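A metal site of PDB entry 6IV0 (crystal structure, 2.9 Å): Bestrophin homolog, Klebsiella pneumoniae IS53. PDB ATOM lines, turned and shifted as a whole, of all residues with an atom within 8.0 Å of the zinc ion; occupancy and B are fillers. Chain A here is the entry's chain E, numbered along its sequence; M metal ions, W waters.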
ATOM      1  N   VAL A  99     -20.563   8.058   6.399  1.00  0.00           N
ATOM      2  CA  VAL A  99     -21.931   8.179   6.859  1.00  0.00           C
ATOM      3  C   VAL A  99     -22.902   8.058   5.689  1.00  0.00           C
ATOM      4  O   VAL A  99     -23.951   7.426   5.815  1.00  0.00           O
ATOM      5  CB  VAL A  99     -22.152   9.475   7.610  1.00  0.00           C
ATOM      6  CG1 VAL A  99     -23.633   9.694   7.928  1.00  0.00           C
ATOM      7  CG2 VAL A  99     -21.285   9.506   8.894  1.00  0.00           C
ATOM      8  N   LEU A 102     -23.244   4.361   5.091  1.00  0.00           N
ATOM      9  CA  LEU A 102     -24.209   3.804   6.063  1.00  0.00           C
ATOM     10  C   LEU A 102     -25.690   4.076   5.708  1.00  0.00           C
ATOM     11  O   LEU A 102     -26.515   3.154   5.758  1.00  0.00           O
ATOM     12  CB  LEU A 102     -23.935   4.339   7.459  1.00  0.00           C
ATOM     13  CG  LEU A 102     -22.782   3.593   8.095  1.00  0.00           C
ATOM     14  CD1 LEU A 102     -22.531   4.165   9.485  1.00  0.00           C
ATOM     15  CD2 LEU A 102     -23.078   2.112   8.129  1.00  0.00           C
ATOM     16  N   ARG A 103     -26.039   5.307   5.340  1.00  0.00           N
ATOM     17  CA  ARG A 103     -27.428   5.579   4.956  1.00  0.00           C
ATOM     18  C   ARG A 103     -27.863   4.832   3.686  1.00  0.00           C
ATOM     19  O   ARG A 103     -28.936   4.255   3.674  1.00  0.00           O
ATOM     20  CB  ARG A 103     -27.677   7.067   4.780  1.00  0.00           C
ATOM     21  CG  ARG A 103     -27.899   7.771   6.092  1.00  0.00           C
ATOM     22  CD  ARG A 103     -28.690   9.050   5.919  1.00  0.00           C
ATOM     23  NE  ARG A 103     -29.984   8.826   5.293  1.00  0.00           N
ATOM     24  CZ  ARG A 103     -30.901   9.771   5.148  1.00  0.00           C
ATOM     25  NH1 ARG A 103     -32.054   9.489   4.552  1.00  0.00           N
ATOM     26  NH2 ARG A 103     -30.652  10.996   5.601  1.00  0.00           N
ATOM     27  N   LEU A 106     -27.528   0.748   4.726  1.00  0.00           N
ATOM     28  CA  LEU A 106     -28.400   0.321   5.815  1.00  0.00           C
ATOM     29  C   LEU A 106     -29.289   1.496   6.219  1.00  0.00           C
ATOM     30  O   LEU A 106     -29.070   2.100   7.269  1.00  0.00           O
ATOM     31  CB  LEU A 106     -27.583  -0.158   7.006  1.00  0.00           C
ATOM     32  CG  LEU A 106     -26.583  -1.243   6.629  1.00  0.00           C
ATOM     33  CD1 LEU A 106     -25.522  -1.462   7.726  1.00  0.00           C
ATOM     34  CD2 LEU A 106     -27.335  -2.491   6.354  1.00  0.00           C
ATOM     35  N   PRO A 107     -30.296   1.826   5.384  1.00  0.00           N
ATOM     36  CA  PRO A 107     -31.107   3.012   5.658  1.00  0.00           C
ATOM     37  C   PRO A 107     -31.926   2.881   6.940  1.00  0.00           C
ATOM     38  O   PRO A 107     -32.197   3.887   7.572  1.00  0.00           O
ATOM     39  CB  PRO A 107     -32.012   3.117   4.421  1.00  0.00           C
ATOM     40  CG  PRO A 107     -31.913   1.837   3.725  1.00  0.00           C
ATOM     41  CD  PRO A 107     -30.677   1.145   4.128  1.00  0.00           C
ATOM     42  N   ALA A 108     -32.249   1.654   7.339  1.00  0.00           N
ATOM     43  CA  ALA A 108     -33.043   1.415   8.540  1.00  0.00           C
ATOM     44  C   ALA A 108     -32.302   1.503   9.879  1.00  0.00           C
ATOM     45  O   ALA A 108     -32.886   1.879  10.892  1.00  0.00           O
ATOM     46  CB  ALA A 108     -33.686   0.071   8.431  1.00  0.00           C
ATOM     47  N   GLU A 109     -31.014   1.203   9.885  1.00  0.00           N
ATOM     48  CA  GLU A 109     -30.298   0.964  11.112  1.00  0.00           C
ATOM     49  C   GLU A 109     -29.833   2.219  11.814  1.00  0.00           C
ATOM     50  O   GLU A 109     -28.673   2.433  12.044  1.00  0.00           O
ATOM     51  CB  GLU A 109     -29.108   0.087  10.788  1.00  0.00           C
ATOM     52  CG  GLU A 109     -29.505  -1.248  10.254  1.00  0.00           C
ATOM     53  CD  GLU A 109     -29.628  -2.286  11.318  1.00  0.00           C
ATOM     54  OE1 GLU A 109     -29.432  -1.965  12.504  1.00  0.00           O
ATOM     55  OE2 GLU A 109     -29.922  -3.434  10.970  1.00  0.00           O
ATOM     56  N   HIS A 110     -30.777   3.033  12.233  1.00  0.00           N
ATOM     57  CA  HIS A 110     -30.423   4.340  12.801  1.00  0.00           C
ATOM     58  C   HIS A 110     -29.690   4.279  14.158  1.00  0.00           C
ATOM     59  O   HIS A 110     -29.021   5.229  14.526  1.00  0.00           O
ATOM     60  CB  HIS A 110     -31.665   5.213  12.948  1.00  0.00           C
ATOM     61  CG  HIS A 110     -32.473   5.324  11.687  1.00  0.00           C
ATOM     62  ND1 HIS A 110     -32.062   6.076  10.599  1.00  0.00           N
ATOM     63  CD2 HIS A 110     -33.663   4.794  11.339  1.00  0.00           C
ATOM     64  CE1 HIS A 110     -32.969   6.002   9.645  1.00  0.00           C
ATOM     65  NE2 HIS A 110     -33.956   5.221  10.072  1.00  0.00           N
ATOM     66  N   ASP A 111     -29.804   3.189  14.901  1.00  0.00           N
ATOM     67  CA  ASP A 111     -29.072   3.115  16.168  1.00  0.00           C
ATOM     68  C   ASP A 111     -27.569   3.043  15.880  1.00  0.00           C
ATOM     69  O   ASP A 111     -26.772   3.725  16.530  1.00  0.00           O
ATOM     70  CB  ASP A 111     -29.519   1.921  17.017  1.00  0.00           C
ATOM     71  CG  ASP A 111     -30.964   2.065  17.522  1.00  0.00           C
ATOM     72  OD1 ASP A 111     -31.520   3.181  17.408  1.00  0.00           O
ATOM     73  OD2 ASP A 111     -31.526   1.073  18.019  1.00  0.00           O
ATOM     74  N   ALA A 112     -27.215   2.208  14.895  1.00  0.00           N
ATOM     75  CA  ALA A 112     -25.846   2.119  14.395  1.00  0.00           C
ATOM     76  C   ALA A 112     -25.385   3.453  13.770  1.00  0.00           C
ATOM     77  O   ALA A 112     -24.248   3.860  13.978  1.00  0.00           O
ATOM     78  CB  ALA A 112     -25.748   0.998  13.381  1.00  0.00           C
ATOM     79  N   HIS A 113     -26.269   4.116  13.023  1.00  0.00           N
ATOM     80  CA  HIS A 113     -25.981   5.423  12.430  1.00  0.00           C
ATOM     81  C   HIS A 113     -25.567   6.416  13.498  1.00  0.00           C
ATOM     82  O   HIS A 113     -24.615   7.185  13.291  1.00  0.00           O
ATOM     83  CB  HIS A 113     -27.185   6.009  11.715  1.00  0.00           C
ATOM     84  CG  HIS A 113     -27.611   5.271  10.487  1.00  0.00           C
ATOM     85  ND1 HIS A 113     -28.688   5.666   9.722  1.00  0.00           N
ATOM     86  CD2 HIS A 113     -27.108   4.169   9.882  1.00  0.00           C
ATOM     87  CE1 HIS A 113     -28.828   4.853   8.697  1.00  0.00           C
ATOM     88  NE2 HIS A 113     -27.883   3.934   8.768  1.00  0.00           N
ATOM     89  N   ARG A 114     -26.257   6.441  14.639  1.00  0.00           N
ATOM     90  CA  ARG A 114     -25.919   7.425  15.639  1.00  0.00           C
ATOM     91  C   ARG A 114     -24.630   7.036  16.380  1.00  0.00           C
ATOM     92  O   ARG A 114     -23.821   7.913  16.734  1.00  0.00           O
ATOM     93  CB  ARG A 114     -27.060   7.657  16.643  1.00  0.00           C
ATOM     94  CG  ARG A 114     -28.439   7.965  16.072  1.00  0.00           C
ATOM     95  CD  ARG A 114     -28.427   8.857  14.807  1.00  0.00           C
ATOM     96  NE  ARG A 114     -29.785   9.091  14.291  1.00  0.00           N
ATOM     97  CZ  ARG A 114     -30.273   8.655  13.119  1.00  0.00           C
ATOM     98  NH1 ARG A 114     -29.522   7.952  12.291  1.00  0.00           N
ATOM     99  NH2 ARG A 114     -31.532   8.941  12.783  1.00  0.00           N
ATOM    100  N   VAL A 117     -21.690   7.794  13.885  1.00  0.00           N
ATOM    101  CA  VAL A 117     -21.494   9.256  13.785  1.00  0.00           C
ATOM    102  C   VAL A 117     -20.886   9.815  15.086  1.00  0.00           C
ATOM    103  O   VAL A 117     -20.134  10.782  15.071  1.00  0.00           O
ATOM    104  CB  VAL A 117     -22.812  10.020  13.442  1.00  0.00           C
ATOM    105  CG1 VAL A 117     -22.604  11.532  13.525  1.00  0.00           C
ATOM    106  CG2 VAL A 117     -23.256   9.670  12.035  1.00  0.00           C
ATOM    107  N   MET A 288     -26.791  14.893   7.932  1.00  0.00           N
ATOM    108  CA  MET A 288     -26.926  13.679   7.121  1.00  0.00           C
ATOM    109  C   MET A 288     -27.752  12.616   7.840  1.00  0.00           C
ATOM    110  O   MET A 288     -28.476  11.862   7.188  1.00  0.00           O
ATOM    111  CB  MET A 288     -25.552  13.104   6.740  1.00  0.00           C
ATOM    112  CG  MET A 288     -24.762  13.945   5.756  1.00  0.00           C
ATOM    113  SD  MET A 288     -23.246  13.147   5.170  1.00  0.00           S
ATOM    114  CE  MET A 288     -24.012  11.672   4.537  1.00  0.00           C
ATOM    115  N   THR A 289     -27.666  12.575   9.171  1.00  0.00           N
ATOM    116  CA  THR A 289     -28.445  11.585   9.906  1.00  0.00           C
ATOM    117  C   THR A 289     -29.759  12.159  10.499  1.00  0.00           C
ATOM    118  O   THR A 289     -30.286  11.686  11.514  1.00  0.00           O
ATOM    119  CB  THR A 289     -27.614  10.970  11.022  1.00  0.00           C
ATOM    120  OG1 THR A 289     -26.981  12.008  11.773  1.00  0.00           O
ATOM    121  CG2 THR A 289     -26.546  10.098  10.418  1.00  0.00           C
ATOM    122  N   GLY A 290     -30.288  13.191   9.838  1.00  0.00           N
ATOM    123  CA  GLY A 290     -31.564  13.757  10.234  1.00  0.00           C
ATOM    124  C   GLY A 290     -31.704  14.321  11.634  1.00  0.00           C
ATOM    125  O   GLY A 290     -32.792  14.728  12.023  1.00  0.00           O
ATOM    126  N   GLN A 291     -30.605  14.417  12.381  1.00  0.00           N
ATOM    127  CA  GLN A 291     -30.687  14.995  13.742  1.00  0.00           C
ATOM    128  C   GLN A 291     -31.143  16.453  13.589  1.00  0.00           C
ATOM    129  O   GLN A 291     -31.676  17.031  14.564  1.00  0.00           O
ATOM    130  CB  GLN A 291     -29.340  14.901  14.454  1.00  0.00           C
ATOM    131  CG  GLN A 291     -28.653  13.562  14.289  1.00  0.00           C
ATOM    132  CD  GLN A 291     -27.855  13.169  15.514  1.00  0.00           C
ATOM    133  OE1 GLN A 291     -27.991  13.769  16.583  1.00  0.00           O
ATOM    134  NE2 GLN A 291     -27.030  12.145  15.372  1.00  0.00           N
HETATM  135 ZN    ZN M   1     -30.114   7.151  10.477  1.00  0.00          ZN
HETATM  136  O   HOH W   1     -30.441   8.441   8.506  1.00  0.00           O
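NH1 of Arg 114 is bound to the zinc ion. A ring nitrogen (ND1) of His 113 binds the zinc ion (2.2 Å). ND1 of His 110 is bound to the zinc ion. The zinc ion is bound by water W1, at 2.4 Å. The zinc ion has four donor atoms within binding distance.
Within 4 Å of the zinc ion: His 110, His 113 and Arg 114. The nearest printed residue that does not touch the zinc ion is Thr 289 (4.6 Å).
NE2 of His 113 lies within hydrogen-bond range of O of Leu 102 (3.4 Å). The guanidinium group (NH2) of Arg 114 lies within hydrogen-bond range of the backbone carbonyl oxygen (O) of Thr 289 (3.3 Å). NE2 of His 110 lies close to O of Pro 107 (3.3 Å). NE2 of His 113 is in hydrogen-bond range of O of Leu 106, 2.6 Å away.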
